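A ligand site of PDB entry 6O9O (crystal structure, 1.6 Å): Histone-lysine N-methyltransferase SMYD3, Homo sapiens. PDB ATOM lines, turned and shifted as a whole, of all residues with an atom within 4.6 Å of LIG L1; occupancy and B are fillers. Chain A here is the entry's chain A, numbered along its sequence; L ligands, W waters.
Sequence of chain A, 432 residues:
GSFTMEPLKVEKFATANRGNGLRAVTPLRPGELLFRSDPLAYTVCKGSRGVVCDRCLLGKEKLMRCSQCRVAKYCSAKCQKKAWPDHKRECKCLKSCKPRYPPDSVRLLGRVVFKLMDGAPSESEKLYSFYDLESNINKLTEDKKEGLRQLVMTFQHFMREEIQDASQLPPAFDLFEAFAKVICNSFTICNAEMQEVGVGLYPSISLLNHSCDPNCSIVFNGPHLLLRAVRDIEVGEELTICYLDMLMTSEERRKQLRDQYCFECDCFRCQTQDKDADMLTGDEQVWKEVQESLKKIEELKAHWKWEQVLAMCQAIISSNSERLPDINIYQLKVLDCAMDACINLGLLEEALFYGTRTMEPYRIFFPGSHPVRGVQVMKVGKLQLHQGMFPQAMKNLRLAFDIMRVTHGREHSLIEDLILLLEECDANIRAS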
ATOM      1  N   CYS A 184      14.348   7.131 -16.002  1.00  0.00           N
ATOM      2  CA  CYS A 184      13.125   6.428 -15.667  1.00  0.00           C
ATOM      3  C   CYS A 184      13.111   5.887 -14.242  1.00  0.00           C
ATOM      4  O   CYS A 184      12.075   5.408 -13.772  1.00  0.00           O
ATOM      5  CB  CYS A 184      12.951   5.324 -16.697  1.00  0.00           C
ATOM      6  SG  CYS A 184      11.966   3.965 -16.192  1.00  0.00           S
ATOM      7  N   ASN A 185      14.249   5.905 -13.537  1.00  0.00           N
ATOM      8  CA  ASN A 185      14.288   5.267 -12.221  1.00  0.00           C
ATOM      9  C   ASN A 185      14.809   6.164 -11.095  1.00  0.00           C
ATOM     10  O   ASN A 185      15.016   5.669  -9.992  1.00  0.00           O
ATOM     11  CB  ASN A 185      15.141   3.988 -12.288  1.00  0.00           C
ATOM     12  CG  ASN A 185      14.474   2.910 -13.117  1.00  0.00           C
ATOM     13  OD1 ASN A 185      13.535   2.261 -12.658  1.00  0.00           O
ATOM     14  ND2 ASN A 185      14.914   2.758 -14.350  1.00  0.00           N
ATOM     15  N   SER A 186      14.997   7.459 -11.348  1.00  0.00           N
ATOM     16  CA  SER A 186      15.437   8.370 -10.297  1.00  0.00           C
ATOM     17  C   SER A 186      14.307   8.676  -9.329  1.00  0.00           C
ATOM     18  O   SER A 186      13.178   8.943  -9.742  1.00  0.00           O
ATOM     19  CB  SER A 186      15.958   9.669 -10.900  1.00  0.00           C
ATOM     20  OG  SER A 186      17.228   9.485 -11.493  1.00  0.00           O
ATOM     21  N   PHE A 187      14.637   8.683  -8.037  1.00  0.00           N
ATOM     22  CA  PHE A 187      13.713   9.091  -6.988  1.00  0.00           C
ATOM     23  C   PHE A 187      14.065  10.486  -6.494  1.00  0.00           C
ATOM     24  O   PHE A 187      15.245  10.796  -6.251  1.00  0.00           O
ATOM     25  CB  PHE A 187      13.765   8.124  -5.806  1.00  0.00           C
ATOM     26  CG  PHE A 187      13.111   6.804  -6.057  1.00  0.00           C
ATOM     27  CD1 PHE A 187      13.792   5.782  -6.714  1.00  0.00           C
ATOM     28  CD2 PHE A 187      11.821   6.566  -5.614  1.00  0.00           C
ATOM     29  CE1 PHE A 187      13.192   4.550  -6.925  1.00  0.00           C
ATOM     30  CE2 PHE A 187      11.200   5.335  -5.835  1.00  0.00           C
ATOM     31  CZ  PHE A 187      11.884   4.329  -6.486  1.00  0.00           C
ATOM     32  N   THR A 188      13.042  11.322  -6.333  1.00  0.00           N
ATOM     33  CA  THR A 188      13.220  12.653  -5.772  1.00  0.00           C
ATOM     34  C   THR A 188      13.155  12.545  -4.242  1.00  0.00           C
ATOM     35  O   THR A 188      12.094  12.265  -3.688  1.00  0.00           O
ATOM     36  CB  THR A 188      12.152  13.603  -6.306  1.00  0.00           C
ATOM     37  OG1 THR A 188      12.284  13.693  -7.741  1.00  0.00           O
ATOM     38  CG2 THR A 188      12.301  14.980  -5.696  1.00  0.00           C
ATOM     39  N   CYS A 190      12.940  13.810  -0.575  1.00  0.00           N
ATOM     40  CA  CYS A 190      12.296  14.963   0.059  1.00  0.00           C
ATOM     41  C   CYS A 190      12.625  15.011   1.543  1.00  0.00           C
ATOM     42  O   CYS A 190      12.713  13.970   2.198  1.00  0.00           O
ATOM     43  CB  CYS A 190      10.774  14.910  -0.137  1.00  0.00           C
ATOM     44  SG  CYS A 190      10.312  14.885  -1.897  1.00  0.00           S
ATOM     45  N   MET A 194       8.883  18.007   3.196  1.00  0.00           N
ATOM     46  CA  MET A 194       8.498  17.704   1.821  1.00  0.00           C
ATOM     47  C   MET A 194       9.116  18.657   0.808  1.00  0.00           C
ATOM     48  O   MET A 194       8.616  18.785  -0.310  1.00  0.00           O
ATOM     49  CB  MET A 194       6.973  17.635   1.679  1.00  0.00           C
ATOM     50  CG  MET A 194       6.400  16.413   2.379  1.00  0.00           C
ATOM     51  SD  MET A 194       6.962  14.884   1.583  1.00  0.00           S
ATOM     52  CE  MET A 194       6.127  13.662   2.602  1.00  0.00           C
ATOM     53  N   GLU A 196      11.982  19.171  -1.839  1.00  0.00           N
ATOM     54  CA  GLU A 196      12.908  18.351  -2.610  1.00  0.00           C
ATOM     55  C   GLU A 196      14.345  18.750  -2.294  1.00  0.00           C
ATOM     56  O   GLU A 196      14.706  19.925  -2.375  1.00  0.00           O
ATOM     57  CB  GLU A 196      12.638  18.530  -4.108  1.00  0.00           C
ATOM     58  CG  GLU A 196      11.193  18.267  -4.514  1.00  0.00           C
ATOM     59  CD  GLU A 196      10.986  18.405  -6.014  1.00  0.00           C
ATOM     60  OE1 GLU A 196      11.966  18.718  -6.733  1.00  0.00           O
ATOM     61  OE2 GLU A 196       9.841  18.191  -6.477  1.00  0.00           O
ATOM     62  N   SER A 206      12.615   0.333  -7.179  1.00  0.00           N
ATOM     63  CA  SER A 206      12.228   0.554  -8.566  1.00  0.00           C
ATOM     64  C   SER A 206      11.337  -0.545  -9.110  1.00  0.00           C
ATOM     65  O   SER A 206      10.823  -0.384 -10.226  1.00  0.00           O
ATOM     66  CB  SER A 206      13.451   0.698  -9.474  1.00  0.00           C
ATOM     67  OG  SER A 206      13.970   2.007  -9.413  1.00  0.00           O
ATOM     68  N   LEU A 208       8.461  -1.161  -8.042  1.00  0.00           N
ATOM     69  CA  LEU A 208       7.076  -0.728  -7.859  1.00  0.00           C
ATOM     70  C   LEU A 208       6.575  -0.026  -9.107  1.00  0.00           C
ATOM     71  O   LEU A 208       7.143   0.988  -9.546  1.00  0.00           O
ATOM     72  CB  LEU A 208       6.968   0.207  -6.661  1.00  0.00           C
ATOM     73  CG  LEU A 208       7.170  -0.427  -5.283  1.00  0.00           C
ATOM     74  CD1 LEU A 208       7.638   0.627  -4.288  1.00  0.00           C
ATOM     75  CD2 LEU A 208       5.869  -1.057  -4.825  1.00  0.00           C
ATOM     76  N   ILE A 218       5.887   5.717  -0.357  1.00  0.00           N
ATOM     77  CA  ILE A 218       7.265   5.845   0.122  1.00  0.00           C
ATOM     78  C   ILE A 218       7.423   7.199   0.793  1.00  0.00           C
ATOM     79  O   ILE A 218       6.736   8.172   0.460  1.00  0.00           O
ATOM     80  CB  ILE A 218       8.312   5.672  -1.000  1.00  0.00           C
ATOM     81  CG1 ILE A 218       8.126   6.766  -2.060  1.00  0.00           C
ATOM     82  CG2 ILE A 218       8.268   4.261  -1.564  1.00  0.00           C
ATOM     83  CD1 ILE A 218       9.257   6.845  -3.091  1.00  0.00           C
ATOM     84  N   PHE A 220      10.789   9.605   2.768  1.00  0.00           N
ATOM     85  CA  PHE A 220      12.219   9.723   3.002  1.00  0.00           C
ATOM     86  C   PHE A 220      12.489  10.256   4.399  1.00  0.00           C
ATOM     87  O   PHE A 220      11.776  11.151   4.880  1.00  0.00           O
ATOM     88  CB  PHE A 220      12.874  10.631   1.955  1.00  0.00           C
ATOM     89  CG  PHE A 220      12.760  10.091   0.565  1.00  0.00           C
ATOM     90  CD1 PHE A 220      13.699   9.184   0.086  1.00  0.00           C
ATOM     91  CD2 PHE A 220      11.690  10.453  -0.245  1.00  0.00           C
ATOM     92  CE1 PHE A 220      13.589   8.663  -1.193  1.00  0.00           C
ATOM     93  CE2 PHE A 220      11.571   9.933  -1.540  1.00  0.00           C
ATOM     94  CZ  PHE A 220      12.528   9.033  -2.015  1.00  0.00           C
ATOM     95  N   ILE A 241       2.945   2.458  -6.168  1.00  0.00           N
ATOM     96  CA  ILE A 241       3.063   3.794  -5.588  1.00  0.00           C
ATOM     97  C   ILE A 241       2.664   4.773  -6.667  1.00  0.00           C
ATOM     98  O   ILE A 241       2.582   4.426  -7.853  1.00  0.00           O
ATOM     99  CB  ILE A 241       4.484   4.108  -5.062  1.00  0.00           C
ATOM    100  CG1 ILE A 241       5.528   3.940  -6.176  1.00  0.00           C
ATOM    101  CG2 ILE A 241       4.808   3.242  -3.854  1.00  0.00           C
ATOM    102  CD1 ILE A 241       6.926   4.420  -5.784  1.00  0.00           C
ATOM    103  N   CYS A 242       2.393   6.013  -6.266  1.00  0.00           N
ATOM    104  CA  CYS A 242       2.162   7.086  -7.217  1.00  0.00           C
ATOM    105  C   CYS A 242       3.484   7.786  -7.488  1.00  0.00           C
ATOM    106  O   CYS A 242       4.094   8.336  -6.563  1.00  0.00           O
ATOM    107  CB  CYS A 242       1.099   8.068  -6.729  1.00  0.00           C
ATOM    108  SG  CYS A 242       0.615   9.277  -7.986  1.00  0.00           S
ATOM    109  N   TYR A 243       3.940   7.761  -8.740  1.00  0.00           N
ATOM    110  CA  TYR A 243       5.195   8.406  -9.107  1.00  0.00           C
ATOM    111  C   TYR A 243       5.124   9.917  -9.024  1.00  0.00           C
ATOM    112  O   TYR A 243       6.168  10.570  -9.067  1.00  0.00           O
ATOM    113  CB  TYR A 243       5.590   8.014 -10.539  1.00  0.00           C
ATOM    114  CG  TYR A 243       5.928   6.558 -10.811  1.00  0.00           C
ATOM    115  CD1 TYR A 243       5.975   5.627  -9.789  1.00  0.00           C
ATOM    116  CD2 TYR A 243       6.222   6.133 -12.104  1.00  0.00           C
ATOM    117  CE1 TYR A 243       6.287   4.298 -10.038  1.00  0.00           C
ATOM    118  CE2 TYR A 243       6.551   4.804 -12.380  1.00  0.00           C
ATOM    119  CZ  TYR A 243       6.581   3.897 -11.330  1.00  0.00           C
ATOM    120  OH  TYR A 243       6.900   2.580 -11.581  1.00  0.00           O
ATOM    121  N   LEU A 244       3.927  10.492  -8.927  1.00  0.00           N
ATOM    122  CA  LEU A 244       3.692  11.897  -9.237  1.00  0.00           C
ATOM    123  C   LEU A 244       3.076  12.666  -8.070  1.00  0.00           C
ATOM    124  O   LEU A 244       2.397  12.100  -7.205  1.00  0.00           O
ATOM    125  CB  LEU A 244       2.744  12.027 -10.441  1.00  0.00           C
ATOM    126  CG  LEU A 244       3.162  11.267 -11.691  1.00  0.00           C
ATOM    127  CD1 LEU A 244       2.083  11.450 -12.738  1.00  0.00           C
ATOM    128  CD2 LEU A 244       4.477  11.860 -12.138  1.00  0.00           C
ATOM    129  N   ASP A 245       3.320  13.972  -8.071  1.00  0.00           N
ATOM    130  CA  ASP A 245       2.568  14.945  -7.279  1.00  0.00           C
ATOM    131  C   ASP A 245       1.069  14.704  -7.459  1.00  0.00           C
ATOM    132  O   ASP A 245       0.599  14.591  -8.593  1.00  0.00           O
ATOM    133  CB  ASP A 245       2.954  16.346  -7.761  1.00  0.00           C
ATOM    134  CG  ASP A 245       2.473  17.480  -6.842  1.00  0.00           C
ATOM    135  OD1 ASP A 245       1.418  17.345  -6.189  1.00  0.00           O
ATOM    136  OD2 ASP A 245       3.157  18.521  -6.812  1.00  0.00           O
ATOM    137  N   TYR A 261       8.481   8.298 -18.275  1.00  0.00           N
ATOM    138  CA  TYR A 261       8.340   6.874 -17.978  1.00  0.00           C
ATOM    139  C   TYR A 261       7.866   6.052 -19.167  1.00  0.00           C
ATOM    140  O   TYR A 261       7.761   4.827 -19.043  1.00  0.00           O
ATOM    141  CB  TYR A 261       7.374   6.681 -16.803  1.00  0.00           C
ATOM    142  CG  TYR A 261       7.894   7.305 -15.526  1.00  0.00           C
ATOM    143  CD1 TYR A 261       8.901   6.692 -14.799  1.00  0.00           C
ATOM    144  CD2 TYR A 261       7.371   8.507 -15.056  1.00  0.00           C
ATOM    145  CE1 TYR A 261       9.373   7.241 -13.623  1.00  0.00           C
ATOM    146  CE2 TYR A 261       7.861   9.084 -13.862  1.00  0.00           C
ATOM    147  CZ  TYR A 261       8.860   8.427 -13.165  1.00  0.00           C
ATOM    148  OH  TYR A 261       9.345   8.976 -11.995  1.00  0.00           O
ATOM    149  N   LEU A 294       3.876  30.126 -11.453  1.00  0.00           N
ATOM    150  CA  LEU A 294       4.375  29.062 -10.587  1.00  0.00           C
ATOM    151  C   LEU A 294       5.671  28.443 -11.094  1.00  0.00           C
ATOM    152  O   LEU A 294       6.391  27.826 -10.304  1.00  0.00           O
ATOM    153  CB  LEU A 294       3.330  27.959 -10.450  1.00  0.00           C
ATOM    154  CG  LEU A 294       2.292  28.135  -9.326  1.00  0.00           C
ATOM    155  CD1 LEU A 294       1.165  27.129  -9.549  1.00  0.00           C
ATOM    156  CD2 LEU A 294       2.912  27.919  -7.953  1.00  0.00           C
ATOM    157  N   GLU A 298       8.225  27.966  -8.226  1.00  0.00           N
ATOM    158  CA  GLU A 298       8.786  26.657  -7.926  1.00  0.00           C
ATOM    159  C   GLU A 298      10.314  26.680  -7.984  1.00  0.00           C
ATOM    160  O   GLU A 298      10.969  26.047  -7.165  1.00  0.00           O
ATOM    161  CB  GLU A 298       8.230  25.620  -8.905  1.00  0.00           C
ATOM    162  CG  GLU A 298       8.777  24.211  -8.704  1.00  0.00           C
ATOM    163  CD  GLU A 298       8.222  23.203  -9.697  1.00  0.00           C
ATOM    164  OE1 GLU A 298       7.818  23.619 -10.807  1.00  0.00           O
ATOM    165  OE2 GLU A 298       8.189  22.002  -9.368  1.00  0.00           O
ATOM    166  N   LYS A 301      11.522  28.447  -4.831  1.00  0.00           N
ATOM    167  CA  LYS A 301      11.378  27.566  -3.685  1.00  0.00           C
ATOM    168  C   LYS A 301      12.446  26.477  -3.686  1.00  0.00           C
ATOM    169  O   LYS A 301      13.012  26.149  -2.635  1.00  0.00           O
ATOM    170  CB  LYS A 301       9.984  26.949  -3.681  1.00  0.00           C
ATOM    171  CG  LYS A 301       9.749  25.915  -2.583  1.00  0.00           C
ATOM    172  CD  LYS A 301       8.302  25.458  -2.546  1.00  0.00           C
ATOM    173  CE  LYS A 301       8.041  24.549  -1.364  1.00  0.00           C
ATOM    174  NZ  LYS A 301       8.620  23.203  -1.580  1.00  0.00           N
ATOM    175  N   LYS A 333      -1.262  25.488  -4.856  1.00  0.00           N
ATOM    176  CA  LYS A 333       0.192  25.451  -4.856  1.00  0.00           C
ATOM    177  C   LYS A 333       0.767  26.769  -4.366  1.00  0.00           C
ATOM    178  O   LYS A 333       1.780  26.784  -3.639  1.00  0.00           O
ATOM    179  CB  LYS A 333       0.693  25.109  -6.258  1.00  0.00           C
ATOM    180  CG  LYS A 333       0.399  23.671  -6.674  1.00  0.00           C
ATOM    181  CD  LYS A 333       0.625  23.503  -8.186  1.00  0.00           C
ATOM    182  CE  LYS A 333       0.118  22.172  -8.713  1.00  0.00           C
ATOM    183  NZ  LYS A 333       1.038  21.049  -8.392  1.00  0.00           N
ATOM    184  N   CYS A 337       3.219  27.193  -1.105  1.00  0.00           N
ATOM    185  CA  CYS A 337       4.520  27.841  -1.149  1.00  0.00           C
ATOM    186  C   CYS A 337       4.561  29.039  -0.216  1.00  0.00           C
ATOM    187  O   CYS A 337       5.564  29.272   0.475  1.00  0.00           O
ATOM    188  CB  CYS A 337       4.851  28.262  -2.579  1.00  0.00           C
ATOM    189  SG  CYS A 337       5.082  26.876  -3.749  1.00  0.00           S
ATOM    190  N   HIS A 370      -1.907   9.766   2.931  1.00  0.00           N
ATOM    191  CA  HIS A 370      -0.848  10.231   2.041  1.00  0.00           C
ATOM    192  C   HIS A 370       0.148  11.025   2.888  1.00  0.00           C
ATOM    193  O   HIS A 370      -0.254  11.918   3.647  1.00  0.00           O
ATOM    194  CB  HIS A 370      -1.400  11.104   0.904  1.00  0.00           C
ATOM    195  CG  HIS A 370      -0.404  11.369  -0.186  1.00  0.00           C
ATOM    196  ND1 HIS A 370       0.704  12.159  -0.010  1.00  0.00           N
ATOM    197  CD2 HIS A 370      -0.393  10.985  -1.482  1.00  0.00           C
ATOM    198  CE1 HIS A 370       1.382  12.235  -1.150  1.00  0.00           C
ATOM    199  NE2 HIS A 370       0.738  11.525  -2.061  1.00  0.00           N
ATOM    200  N   VAL A 372       2.095  13.488   2.271  1.00  0.00           N
ATOM    201  CA  VAL A 372       2.136  14.928   2.055  1.00  0.00           C
ATOM    202  C   VAL A 372       1.001  15.613   2.830  1.00  0.00           C
ATOM    203  O   VAL A 372       1.199  16.691   3.401  1.00  0.00           O
ATOM    204  CB  VAL A 372       2.080  15.255   0.550  1.00  0.00           C
ATOM    205  CG1 VAL A 372       1.735  16.718   0.334  1.00  0.00           C
ATOM    206  CG2 VAL A 372       3.428  14.915  -0.102  1.00  0.00           C
HETATM  207  C1  LIG L   1       5.133  18.107  -3.958  1.00  0.00           C
HETATM  208  C2  LIG L   1       6.408  14.885  -2.247  1.00  0.00           C
HETATM  209  C3  LIG L   1       7.985  11.417  -6.037  1.00  0.00           C
HETATM  210  C4  LIG L   1       6.520  11.779  -6.135  1.00  0.00           C
HETATM  211  C5  LIG L   1       6.241  13.042  -5.348  1.00  0.00           C
HETATM  212  C6  LIG L   1       9.374   9.720  -7.126  1.00  0.00           C
HETATM  213  C7  LIG L   1       9.347   8.357  -7.718  1.00  0.00           C
HETATM  214  C8  LIG L   1       9.754   6.601  -8.914  1.00  0.00           C
HETATM  215  C9  LIG L   1       5.112  24.155  -7.051  1.00  0.00           C
HETATM  216  C10 LIG L   1       4.730  22.933  -6.311  1.00  0.00           C
HETATM  217  C11 LIG L   1       5.892  22.018  -6.050  1.00  0.00           C
HETATM  218  C12 LIG L   1       5.549  20.979  -5.004  1.00  0.00           C
HETATM  219  C13 LIG L   1       6.431  18.878  -4.037  1.00  0.00           C
HETATM  220  C14 LIG L   1       5.207  16.946  -2.970  1.00  0.00           C
HETATM  221  C15 LIG L   1       6.337  15.993  -3.303  1.00  0.00           C
HETATM  222  C16 LIG L   1       8.087  12.581  -3.817  1.00  0.00           C
HETATM  223  C17 LIG L   1       8.449  11.321  -4.583  1.00  0.00           C
HETATM  224  C18 LIG L   1      10.186   7.844  -8.716  1.00  0.00           C
HETATM  225  C19 LIG L   1      10.373   5.671  -9.909  1.00  0.00           C
HETATM  226  C20 LIG L   1       7.646  16.779  -3.303  1.00  0.00           C
HETATM  227  C21 LIG L   1       7.608  17.954  -4.283  1.00  0.00           C
HETATM  228  F1  LIG L   1       6.170  24.773  -6.532  1.00  0.00           F
HETATM  229  F2  LIG L   1       5.404  23.945  -8.305  1.00  0.00           F
HETATM  230  F3  LIG L   1       4.125  25.029  -7.047  1.00  0.00           F
HETATM  231  N1  LIG L   1       6.314  19.739  -5.219  1.00  0.00           N
HETATM  232  N2  LIG L   1       6.643  12.813  -3.963  1.00  0.00           N
HETATM  233  N3  LIG L   1       8.180  10.130  -6.680  1.00  0.00           N
HETATM  234  N4  LIG L   1       8.432   7.481  -7.330  1.00  0.00           N
HETATM  235  O1  LIG L   1       5.858  12.406  -1.663  1.00  0.00           O
HETATM  236  O2  LIG L   1       4.395  13.560  -3.286  1.00  0.00           O
HETATM  237  O3  LIG L   1      10.397  10.395  -7.059  1.00  0.00           O
HETATM  238  O4  LIG L   1       8.700   6.317  -8.108  1.00  0.00           O
HETATM  239  S1  LIG L   1       5.702  13.332  -2.738  1.00  0.00           S
HETATM  240  C22 LIG L   1       9.654   5.138 -11.109  1.00  0.00           C
HETATM  241  C23 LIG L   1       9.936   4.226  -9.979  1.00  0.00           C
HETATM  242  N1  LG2 L   2       8.072  -2.252 -14.595  1.00  0.00           N
HETATM  243  C1  LG2 L   2       9.390  -1.755 -14.173  1.00  0.00           C
HETATM  244  C2  LG2 L   2       9.370  -1.378 -12.702  1.00  0.00           C
HETATM  245  C3  LG2 L   2       8.884   0.065 -12.494  1.00  0.00           C
HETATM  246  S1  LG2 L   2      10.115   1.230 -13.151  1.00  0.00           S
HETATM  247  C4  LG2 L   2      10.479  -2.773 -14.492  1.00  0.00           C
HETATM  248  O1  LG2 L   2      11.629  -2.620 -14.093  1.00  0.00           O
HETATM  249  O2  LG2 L   2      10.213  -3.771 -15.175  1.00  0.00           O
HETATM  250  C5  LG2 L   2       9.016   2.266 -14.172  1.00  0.00           C
HETATM  251  C6  LG2 L   2       8.652   1.677 -15.533  1.00  0.00           C
HETATM  252  O3  LG2 L   2       7.720   0.645 -15.337  1.00  0.00           O
HETATM  253  C7  LG2 L   2       7.949   2.671 -16.447  1.00  0.00           C
HETATM  254  O4  LG2 L   2       8.885   3.434 -17.197  1.00  0.00           O
HETATM  255  C8  LG2 L   2       7.100   1.772 -17.304  1.00  0.00           C
HETATM  256  O5  LG2 L   2       7.925   1.103 -18.233  1.00  0.00           O
HETATM  257  C9  LG2 L   2       6.686   0.735 -16.298  1.00  0.00           C
HETATM  258  N2  LG2 L   2       5.440   1.088 -15.576  1.00  0.00           N
HETATM  259  C10 LG2 L   2       5.335   1.568 -14.292  1.00  0.00           C
HETATM  260  N3  LG2 L   2       4.017   1.741 -13.995  1.00  0.00           N
HETATM  261  C11 LG2 L   2       3.299   1.367 -15.094  1.00  0.00           C
HETATM  262  C12 LG2 L   2       1.937   1.346 -15.381  1.00  0.00           C
HETATM  263  N4  LG2 L   2       1.017   1.711 -14.487  1.00  0.00           N
HETATM  264  N5  LG2 L   2       1.534   0.923 -16.625  1.00  0.00           N
HETATM  265  C13 LG2 L   2       2.438   0.518 -17.577  1.00  0.00           C
HETATM  266  N6  LG2 L   2       3.780   0.544 -17.311  1.00  0.00           N
HETATM  267  C14 LG2 L   2       4.188   0.967 -16.090  1.00  0.00           C
HETATM  268  O   HOH W   1       1.770  14.605  -3.770  1.00  0.00           O
HETATM  269  O   HOH W   2       1.828  17.360  -3.469  1.00  0.00           O
HETATM  270  O   HOH W   3       6.858  10.977   0.609  1.00  0.00           O
HETATM  271  O   HOH W   4       2.096  20.707  -5.763  1.00  0.00           O
HETATM  272  O   HOH W   5      11.454  11.452 -10.027  1.00  0.00           O
HETATM  273  O   HOH W   6       8.545  22.140  -4.271  1.00  0.00           O
HETATM  274  O   HOH W   7       6.940  20.751  -1.166  1.00  0.00           O
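O of Tyr 243 lies within hydrogen-bond range of N3 of LIG L1 (3.2 Å). OD2 of Asp 245 lies within salt-bridge range of N1 of LIG L1 (3.7 Å). A sulfur (S1) of LG2 L2 lies close to the side-chain amide oxygen (OD1) of Asn 185 (3.6 Å). An oxygen (O4) of LG2 L2 sits at hydrogen-bond distance from the side-chain sulfur of Cys 184. O of Tyr 261 sits at hydrogen-bond distance from O4 of LG2 L2, 2.6 Å away. O3 of LIG L1 lies within hydrogen-bond range of N of Thr 188 (2.9 Å).
The side-chain sulfur of Cys 337 is in hydrogen-bond range of the backbone carbonyl oxygen of Lys 333 (3.3 Å). O of Thr 188 sits at hydrogen-bond distance from SG of Cys 190, at 3.6 Å. A ring nitrogen (ND1) of His 370 is in hydrogen-bond range of the backbone NH (N) of Val 372 (3.0 Å). The side-chain hydroxyl of Tyr 243 is in hydrogen-bond range of the backbone carbonyl oxygen of Leu 208 (2.6 Å). The side-chain amide nitrogen of Asn 185 lies close to the side-chain sulfur of Cys 184 (3.7 Å). OD2 of Asp 245 is in salt-bridge range of NZ of Lys 333 (3.7 Å).
The side-chain carboxylate of Glu 298 lies close to a fluorine (F2) of LIG L1, 3.5 Å away. The side-chain sulfur (SG) of Cys 337 sits close to a fluorine (F1) of LIG L1, 3.7 Å away. Merely in contact with LIG L1: Cys 184, Ser 186, Phe 187, Cys 190, Met 194, Glu 196, Ile 241, Tyr 261, Leu 294, Lys 333, His 370 and Val 372. Hydrophobic or aromatic side chains within 4 Å of LIG L1: Phe 187, Met 194, Ile 241, Tyr 243, Tyr 261, Leu 294, His 370 and Val 372. Of the 25 residues printed, 17 come within 4 Å of LIG L1.
Water W3 bridges O of Ile 218 and O1 of LIG L1. Water W6 bridges NZ of Lys 301 (2.9 Å) and N1 of LIG L1 (3.4 Å). Water W5 lies within hydrogen-bond range of O of Ser 186 (3.1 Å), OG1 of Thr 188 (3.3 Å) and O3 of LIG L1 (3.3 Å). Water W7 lies within hydrogen-bond range of O of Met 194 and NZ of Lys 301. Water W4 lies within hydrogen-bond range of the side-chain carboxylate (OD2) of Asp 245 and the side-chain amino group (NZ) of Lys 333.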
